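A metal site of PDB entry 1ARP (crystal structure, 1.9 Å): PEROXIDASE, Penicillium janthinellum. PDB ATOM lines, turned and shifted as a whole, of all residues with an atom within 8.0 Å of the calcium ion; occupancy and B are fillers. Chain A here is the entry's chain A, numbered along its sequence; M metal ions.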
ATOM      1  N   PRO A 130       7.314  18.499 -26.700  1.00  0.00           N
ATOM      2  CA  PRO A 130       6.515  19.046 -25.617  1.00  0.00           C
ATOM      3  C   PRO A 130       5.647  18.019 -24.945  1.00  0.00           C
ATOM      4  O   PRO A 130       5.038  17.186 -25.623  1.00  0.00           O
ATOM      5  CB  PRO A 130       5.692  20.111 -26.229  1.00  0.00           C
ATOM      6  CG  PRO A 130       6.497  20.519 -27.411  1.00  0.00           C
ATOM      7  CD  PRO A 130       7.069  19.227 -27.926  1.00  0.00           C
ATOM      8  N   ALA A 182       1.741   4.746 -25.478  1.00  0.00           N
ATOM      9  CA  ALA A 182       1.656   6.189 -25.427  1.00  0.00           C
ATOM     10  C   ALA A 182       2.582   6.761 -26.498  1.00  0.00           C
ATOM     11  O   ALA A 182       2.354   7.845 -26.990  1.00  0.00           O
ATOM     12  CB  ALA A 182       2.074   6.707 -24.065  1.00  0.00           C
ATOM     13  N   ALA A 183       3.589   6.014 -26.956  1.00  0.00           N
ATOM     14  CA  ALA A 183       4.462   6.438 -28.017  1.00  0.00           C
ATOM     15  C   ALA A 183       3.755   6.644 -29.345  1.00  0.00           C
ATOM     16  O   ALA A 183       4.258   7.384 -30.193  1.00  0.00           O
ATOM     17  CB  ALA A 183       5.507   5.417 -28.218  1.00  0.00           C
ATOM     18  N   HIS A 184       2.563   6.094 -29.594  1.00  0.00           N
ATOM     19  CA  HIS A 184       1.880   6.369 -30.832  1.00  0.00           C
ATOM     20  C   HIS A 184       1.241   7.768 -30.804  1.00  0.00           C
ATOM     21  O   HIS A 184       0.596   8.259 -31.727  1.00  0.00           O
ATOM     22  CB  HIS A 184       0.834   5.271 -31.088  1.00  0.00           C
ATOM     23  CG  HIS A 184       1.344   4.000 -31.761  1.00  0.00           C
ATOM     24  ND1 HIS A 184       0.544   3.049 -32.369  1.00  0.00           N
ATOM     25  CD2 HIS A 184       2.675   3.639 -31.893  1.00  0.00           C
ATOM     26  CE1 HIS A 184       1.367   2.130 -32.892  1.00  0.00           C
ATOM     27  NE2 HIS A 184       2.584   2.434 -32.632  1.00  0.00           N
ATOM     28  N   SER A 185       1.496   8.518 -29.719  1.00  0.00           N
ATOM     29  CA  SER A 185       1.099   9.895 -29.609  1.00  0.00           C
ATOM     30  C   SER A 185       2.096  10.741 -30.403  1.00  0.00           C
ATOM     31  O   SER A 185       1.821  11.916 -30.593  1.00  0.00           O
ATOM     32  CB  SER A 185       1.145  10.293 -28.168  1.00  0.00           C
ATOM     33  OG  SER A 185       0.549  11.548 -27.945  1.00  0.00           O
ATOM     34  N   LEU A 186       3.305  10.258 -30.756  1.00  0.00           N
ATOM     35  CA  LEU A 186       4.289  11.023 -31.484  1.00  0.00           C
ATOM     36  C   LEU A 186       4.473  10.172 -32.716  1.00  0.00           C
ATOM     37  O   LEU A 186       5.573   9.667 -32.961  1.00  0.00           O
ATOM     38  CB  LEU A 186       5.486  11.070 -30.591  1.00  0.00           C
ATOM     39  CG  LEU A 186       5.917  12.306 -29.763  1.00  0.00           C
ATOM     40  CD1 LEU A 186       4.773  13.227 -29.451  1.00  0.00           C
ATOM     41  CD2 LEU A 186       6.606  11.791 -28.518  1.00  0.00           C
ATOM     42  N   ALA A 187       3.478  10.049 -33.564  1.00  0.00           N
ATOM     43  CA  ALA A 187       3.610   9.043 -34.617  1.00  0.00           C
ATOM     44  C   ALA A 187       2.937   9.177 -35.955  1.00  0.00           C
ATOM     45  O   ALA A 187       1.921   9.873 -36.018  1.00  0.00           O
ATOM     46  CB  ALA A 187       3.161   7.711 -34.060  1.00  0.00           C
ATOM     47  N   PRO A 200      -0.438  11.339 -39.522  1.00  0.00           N
ATOM     48  CA  PRO A 200      -0.331  11.164 -38.071  1.00  0.00           C
ATOM     49  C   PRO A 200      -1.314  10.144 -37.523  1.00  0.00           C
ATOM     50  O   PRO A 200      -2.364   9.866 -38.104  1.00  0.00           O
ATOM     51  CB  PRO A 200      -0.576  12.542 -37.486  1.00  0.00           C
ATOM     52  CG  PRO A 200      -0.369  13.487 -38.613  1.00  0.00           C
ATOM     53  CD  PRO A 200      -0.908  12.707 -39.803  1.00  0.00           C
ATOM     54  N   LEU A 201      -0.935   9.526 -36.414  1.00  0.00           N
ATOM     55  CA  LEU A 201      -1.837   8.598 -35.752  1.00  0.00           C
ATOM     56  C   LEU A 201      -2.680   9.374 -34.722  1.00  0.00           C
ATOM     57  O   LEU A 201      -3.650   8.839 -34.201  1.00  0.00           O
ATOM     58  CB  LEU A 201      -0.995   7.480 -35.155  1.00  0.00           C
ATOM     59  CG  LEU A 201      -0.742   6.224 -36.019  1.00  0.00           C
ATOM     60  CD1 LEU A 201      -0.731   6.508 -37.495  1.00  0.00           C
ATOM     61  CD2 LEU A 201       0.581   5.657 -35.630  1.00  0.00           C
ATOM     62  N   ASP A 202      -2.385  10.602 -34.344  1.00  0.00           N
ATOM     63  CA  ASP A 202      -3.297  11.377 -33.524  1.00  0.00           C
ATOM     64  C   ASP A 202      -3.170  12.820 -34.046  1.00  0.00           C
ATOM     65  O   ASP A 202      -2.233  13.092 -34.798  1.00  0.00           O
ATOM     66  CB  ASP A 202      -2.968  11.290 -32.002  1.00  0.00           C
ATOM     67  CG  ASP A 202      -1.831  12.035 -31.298  1.00  0.00           C
ATOM     68  OD1 ASP A 202      -0.971  12.645 -31.919  1.00  0.00           O
ATOM     69  OD2 ASP A 202      -1.790  11.974 -30.082  1.00  0.00           O
ATOM     70  N   SER A 203      -3.962  13.798 -33.612  1.00  0.00           N
ATOM     71  CA  SER A 203      -3.867  15.109 -34.218  1.00  0.00           C
ATOM     72  C   SER A 203      -2.729  15.994 -33.732  1.00  0.00           C
ATOM     73  O   SER A 203      -2.631  17.171 -34.077  1.00  0.00           O
ATOM     74  CB  SER A 203      -5.197  15.781 -34.019  1.00  0.00           C
ATOM     75  OG  SER A 203      -5.461  15.979 -32.629  1.00  0.00           O
ATOM     76  N   THR A 204      -1.828  15.452 -32.916  1.00  0.00           N
ATOM     77  CA  THR A 204      -0.711  16.236 -32.404  1.00  0.00           C
ATOM     78  C   THR A 204       0.562  15.376 -32.446  1.00  0.00           C
ATOM     79  O   THR A 204       1.078  15.039 -31.381  1.00  0.00           O
ATOM     80  CB  THR A 204      -1.067  16.693 -30.977  1.00  0.00           C
ATOM     81  OG1 THR A 204      -1.495  15.562 -30.220  1.00  0.00           O
ATOM     82  CG2 THR A 204      -2.169  17.735 -30.969  1.00  0.00           C
ATOM     83  N   PRO A 205       1.140  15.001 -33.619  1.00  0.00           N
ATOM     84  CA  PRO A 205       2.269  14.124 -33.710  1.00  0.00           C
ATOM     85  C   PRO A 205       3.548  14.706 -33.174  1.00  0.00           C
ATOM     86  O   PRO A 205       4.574  13.996 -33.130  1.00  0.00           O
ATOM     87  CB  PRO A 205       2.341  13.764 -35.160  1.00  0.00           C
ATOM     88  CG  PRO A 205       1.877  15.032 -35.826  1.00  0.00           C
ATOM     89  CD  PRO A 205       0.664  15.352 -34.959  1.00  0.00           C
ATOM     90  N   GLN A 206       3.467  15.992 -32.777  1.00  0.00           N
ATOM     91  CA  GLN A 206       4.625  16.621 -32.141  1.00  0.00           C
ATOM     92  C   GLN A 206       4.387  16.922 -30.675  1.00  0.00           C
ATOM     93  O   GLN A 206       5.192  17.586 -30.064  1.00  0.00           O
ATOM     94  CB  GLN A 206       4.984  17.907 -32.858  1.00  0.00           C
ATOM     95  CG  GLN A 206       5.649  17.645 -34.176  1.00  0.00           C
ATOM     96  CD  GLN A 206       6.265  18.902 -34.786  1.00  0.00           C
ATOM     97  OE1 GLN A 206       5.597  19.743 -35.378  1.00  0.00           O
ATOM     98  NE2 GLN A 206       7.570  19.073 -34.706  1.00  0.00           N
ATOM     99  N   VAL A 207       3.312  16.490 -30.050  1.00  0.00           N
ATOM    100  CA  VAL A 207       3.033  16.754 -28.646  1.00  0.00           C
ATOM    101  C   VAL A 207       2.739  15.412 -27.969  1.00  0.00           C
ATOM    102  O   VAL A 207       1.907  14.624 -28.433  1.00  0.00           O
ATOM    103  CB  VAL A 207       1.815  17.702 -28.479  1.00  0.00           C
ATOM    104  CG1 VAL A 207       1.620  18.005 -27.009  1.00  0.00           C
ATOM    105  CG2 VAL A 207       2.024  19.020 -29.190  1.00  0.00           C
ATOM    106  N   PHE A 208       3.441  15.110 -26.890  1.00  0.00           N
ATOM    107  CA  PHE A 208       3.256  13.884 -26.174  1.00  0.00           C
ATOM    108  C   PHE A 208       2.153  14.211 -25.202  1.00  0.00           C
ATOM    109  O   PHE A 208       2.348  14.830 -24.162  1.00  0.00           O
ATOM    110  CB  PHE A 208       4.537  13.503 -25.479  1.00  0.00           C
ATOM    111  CG  PHE A 208       4.426  12.123 -24.824  1.00  0.00           C
ATOM    112  CD1 PHE A 208       4.434  10.997 -25.590  1.00  0.00           C
ATOM    113  CD2 PHE A 208       4.323  12.014 -23.454  1.00  0.00           C
ATOM    114  CE1 PHE A 208       4.342   9.777 -24.974  1.00  0.00           C
ATOM    115  CE2 PHE A 208       4.233  10.799 -22.846  1.00  0.00           C
ATOM    116  CZ  PHE A 208       4.245   9.686 -23.613  1.00  0.00           C
ATOM    117  N   ASP A 209       0.968  13.755 -25.586  1.00  0.00           N
ATOM    118  CA  ASP A 209      -0.245  14.016 -24.881  1.00  0.00           C
ATOM    119  C   ASP A 209      -1.192  12.834 -25.058  1.00  0.00           C
ATOM    120  O   ASP A 209      -0.979  11.947 -25.895  1.00  0.00           O
ATOM    121  CB  ASP A 209      -0.895  15.248 -25.437  1.00  0.00           C
ATOM    122  CG  ASP A 209      -1.247  15.236 -26.920  1.00  0.00           C
ATOM    123  OD1 ASP A 209      -1.128  14.226 -27.596  1.00  0.00           O
ATOM    124  OD2 ASP A 209      -1.656  16.269 -27.422  1.00  0.00           O
ATOM    125  N   THR A 210      -2.307  12.921 -24.407  1.00  0.00           N
ATOM    126  CA  THR A 210      -3.364  11.958 -24.380  1.00  0.00           C
ATOM    127  C   THR A 210      -4.186  11.772 -25.668  1.00  0.00           C
ATOM    128  O   THR A 210      -4.840  10.751 -25.824  1.00  0.00           O
ATOM    129  CB  THR A 210      -4.040  12.529 -23.114  1.00  0.00           C
ATOM    130  OG1 THR A 210      -3.866  11.579 -22.082  1.00  0.00           O
ATOM    131  CG2 THR A 210      -5.393  13.009 -23.409  1.00  0.00           C
ATOM    132  N   GLN A 211      -4.197  12.716 -26.623  1.00  0.00           N
ATOM    133  CA  GLN A 211      -5.036  12.670 -27.825  1.00  0.00           C
ATOM    134  C   GLN A 211      -5.128  11.346 -28.568  1.00  0.00           C
ATOM    135  O   GLN A 211      -6.183  11.013 -29.087  1.00  0.00           O
ATOM    136  CB  GLN A 211      -4.581  13.711 -28.829  1.00  0.00           C
ATOM    137  CG  GLN A 211      -4.790  15.142 -28.433  1.00  0.00           C
ATOM    138  CD  GLN A 211      -6.195  15.516 -27.969  1.00  0.00           C
ATOM    139  OE1 GLN A 211      -6.355  16.147 -26.921  1.00  0.00           O
ATOM    140  NE2 GLN A 211      -7.259  15.183 -28.679  1.00  0.00           N
ATOM    141  N   PHE A 212      -4.065  10.550 -28.567  1.00  0.00           N
ATOM    142  CA  PHE A 212      -4.012   9.270 -29.230  1.00  0.00           C
ATOM    143  C   PHE A 212      -5.035   8.314 -28.641  1.00  0.00           C
ATOM    144  O   PHE A 212      -5.755   7.626 -29.361  1.00  0.00           O
ATOM    145  CB  PHE A 212      -2.590   8.710 -29.100  1.00  0.00           C
ATOM    146  CG  PHE A 212      -2.557   7.245 -29.443  1.00  0.00           C
ATOM    147  CD1 PHE A 212      -2.747   6.836 -30.730  1.00  0.00           C
ATOM    148  CD2 PHE A 212      -2.383   6.332 -28.411  1.00  0.00           C
ATOM    149  CE1 PHE A 212      -2.780   5.479 -31.001  1.00  0.00           C
ATOM    150  CE2 PHE A 212      -2.421   4.991 -28.686  1.00  0.00           C
ATOM    151  CZ  PHE A 212      -2.608   4.550 -29.981  1.00  0.00           C
ATOM    152  N   TYR A 213      -5.130   8.284 -27.315  1.00  0.00           N
ATOM    153  CA  TYR A 213      -6.070   7.412 -26.655  1.00  0.00           C
ATOM    154  C   TYR A 213      -7.481   7.910 -26.945  1.00  0.00           C
ATOM    155  O   TYR A 213      -8.339   7.093 -27.239  1.00  0.00           O
ATOM    156  CB  TYR A 213      -5.731   7.412 -25.171  1.00  0.00           C
ATOM    157  CG  TYR A 213      -4.413   6.686 -24.888  1.00  0.00           C
ATOM    158  CD1 TYR A 213      -4.360   5.308 -24.832  1.00  0.00           C
ATOM    159  CD2 TYR A 213      -3.267   7.416 -24.638  1.00  0.00           C
ATOM    160  CE1 TYR A 213      -3.186   4.635 -24.539  1.00  0.00           C
ATOM    161  CE2 TYR A 213      -2.100   6.761 -24.335  1.00  0.00           C
ATOM    162  CZ  TYR A 213      -2.066   5.388 -24.283  1.00  0.00           C
ATOM    163  OH  TYR A 213      -0.889   4.788 -23.954  1.00  0.00           O
ATOM    164  N   GLU A 215      -8.565   9.719 -29.661  1.00  0.00           N
ATOM    165  CA  GLU A 215      -8.938   9.610 -31.053  1.00  0.00           C
ATOM    166  C   GLU A 215      -9.056   8.245 -31.644  1.00  0.00           C
ATOM    167  O   GLU A 215      -9.793   8.104 -32.612  1.00  0.00           O
ATOM    168  CB  GLU A 215      -7.985  10.482 -31.857  1.00  0.00           C
ATOM    169  CG  GLU A 215      -8.204  11.975 -31.548  1.00  0.00           C
ATOM    170  CD  GLU A 215      -7.091  12.894 -31.981  1.00  0.00           C
ATOM    171  OE1 GLU A 215      -6.273  12.565 -32.817  1.00  0.00           O
ATOM    172  OE2 GLU A 215      -7.047  13.985 -31.456  1.00  0.00           O
ATOM    173  N   ASN A 266      -2.557  13.837 -18.871  1.00  0.00           N
ATOM    174  CA  ASN A 266      -1.235  13.746 -19.440  1.00  0.00           C
ATOM    175  C   ASN A 266      -0.267  13.361 -18.336  1.00  0.00           C
ATOM    176  O   ASN A 266       0.707  12.671 -18.571  1.00  0.00           O
ATOM    177  CB  ASN A 266      -0.804  15.077 -20.079  1.00  0.00           C
ATOM    178  CG  ASN A 266      -1.595  15.412 -21.327  1.00  0.00           C
ATOM    179  OD1 ASN A 266      -1.723  14.591 -22.215  1.00  0.00           O
ATOM    180  ND2 ASN A 266      -2.203  16.566 -21.447  1.00  0.00           N
ATOM    181  N   MET A 269      -0.697   9.423 -17.776  1.00  0.00           N
ATOM    182  CA  MET A 269      -0.112   8.752 -18.915  1.00  0.00           C
ATOM    183  C   MET A 269       1.406   8.853 -18.906  1.00  0.00           C
ATOM    184  O   MET A 269       2.114   7.884 -19.140  1.00  0.00           O
ATOM    185  CB  MET A 269      -0.654   9.369 -20.180  1.00  0.00           C
ATOM    186  CG  MET A 269       0.062   8.788 -21.388  1.00  0.00           C
ATOM    187  SD  MET A 269      -0.263   9.769 -22.851  1.00  0.00           S
ATOM    188  CE  MET A 269       0.655  11.212 -22.391  1.00  0.00           C
ATOM    189  N   ASN A 303       3.632  20.927 -21.709  1.00  0.00           N
ATOM    190  CA  ASN A 303       2.499  21.040 -22.599  1.00  0.00           C
ATOM    191  C   ASN A 303       1.363  21.587 -21.757  1.00  0.00           C
ATOM    192  O   ASN A 303       1.017  20.996 -20.734  1.00  0.00           O
ATOM    193  CB  ASN A 303       2.123  19.689 -23.135  1.00  0.00           C
ATOM    194  CG  ASN A 303       0.777  19.724 -23.815  1.00  0.00           C
ATOM    195  OD1 ASN A 303       0.353  20.713 -24.425  1.00  0.00           O
ATOM    196  ND2 ASN A 303       0.084  18.625 -23.675  1.00  0.00           N
HETATM  197 CA    CA M   1       0.111  13.499 -29.711  1.00  0.00          CA
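The calcium ion is bound by OD2 of Asp 202 (2.5 Å), O of Thr 204 (2.5 Å), O of Val 207 (2.5 Å), O of Ser 185 (2.5 Å), OD1 of Asp 209 (2.6 Å), OD1 of Asp 202 (2.6 Å), OG1 of Thr 204 (2.7 Å) and OG of Ser 185 (2.7 Å).
Of the 25 residues printed, 5 come within 4 Å of the calcium ion.
The side-chain carboxylate of Asp 202 lies close to the backbone NH of Phe 212 (3.1 Å).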
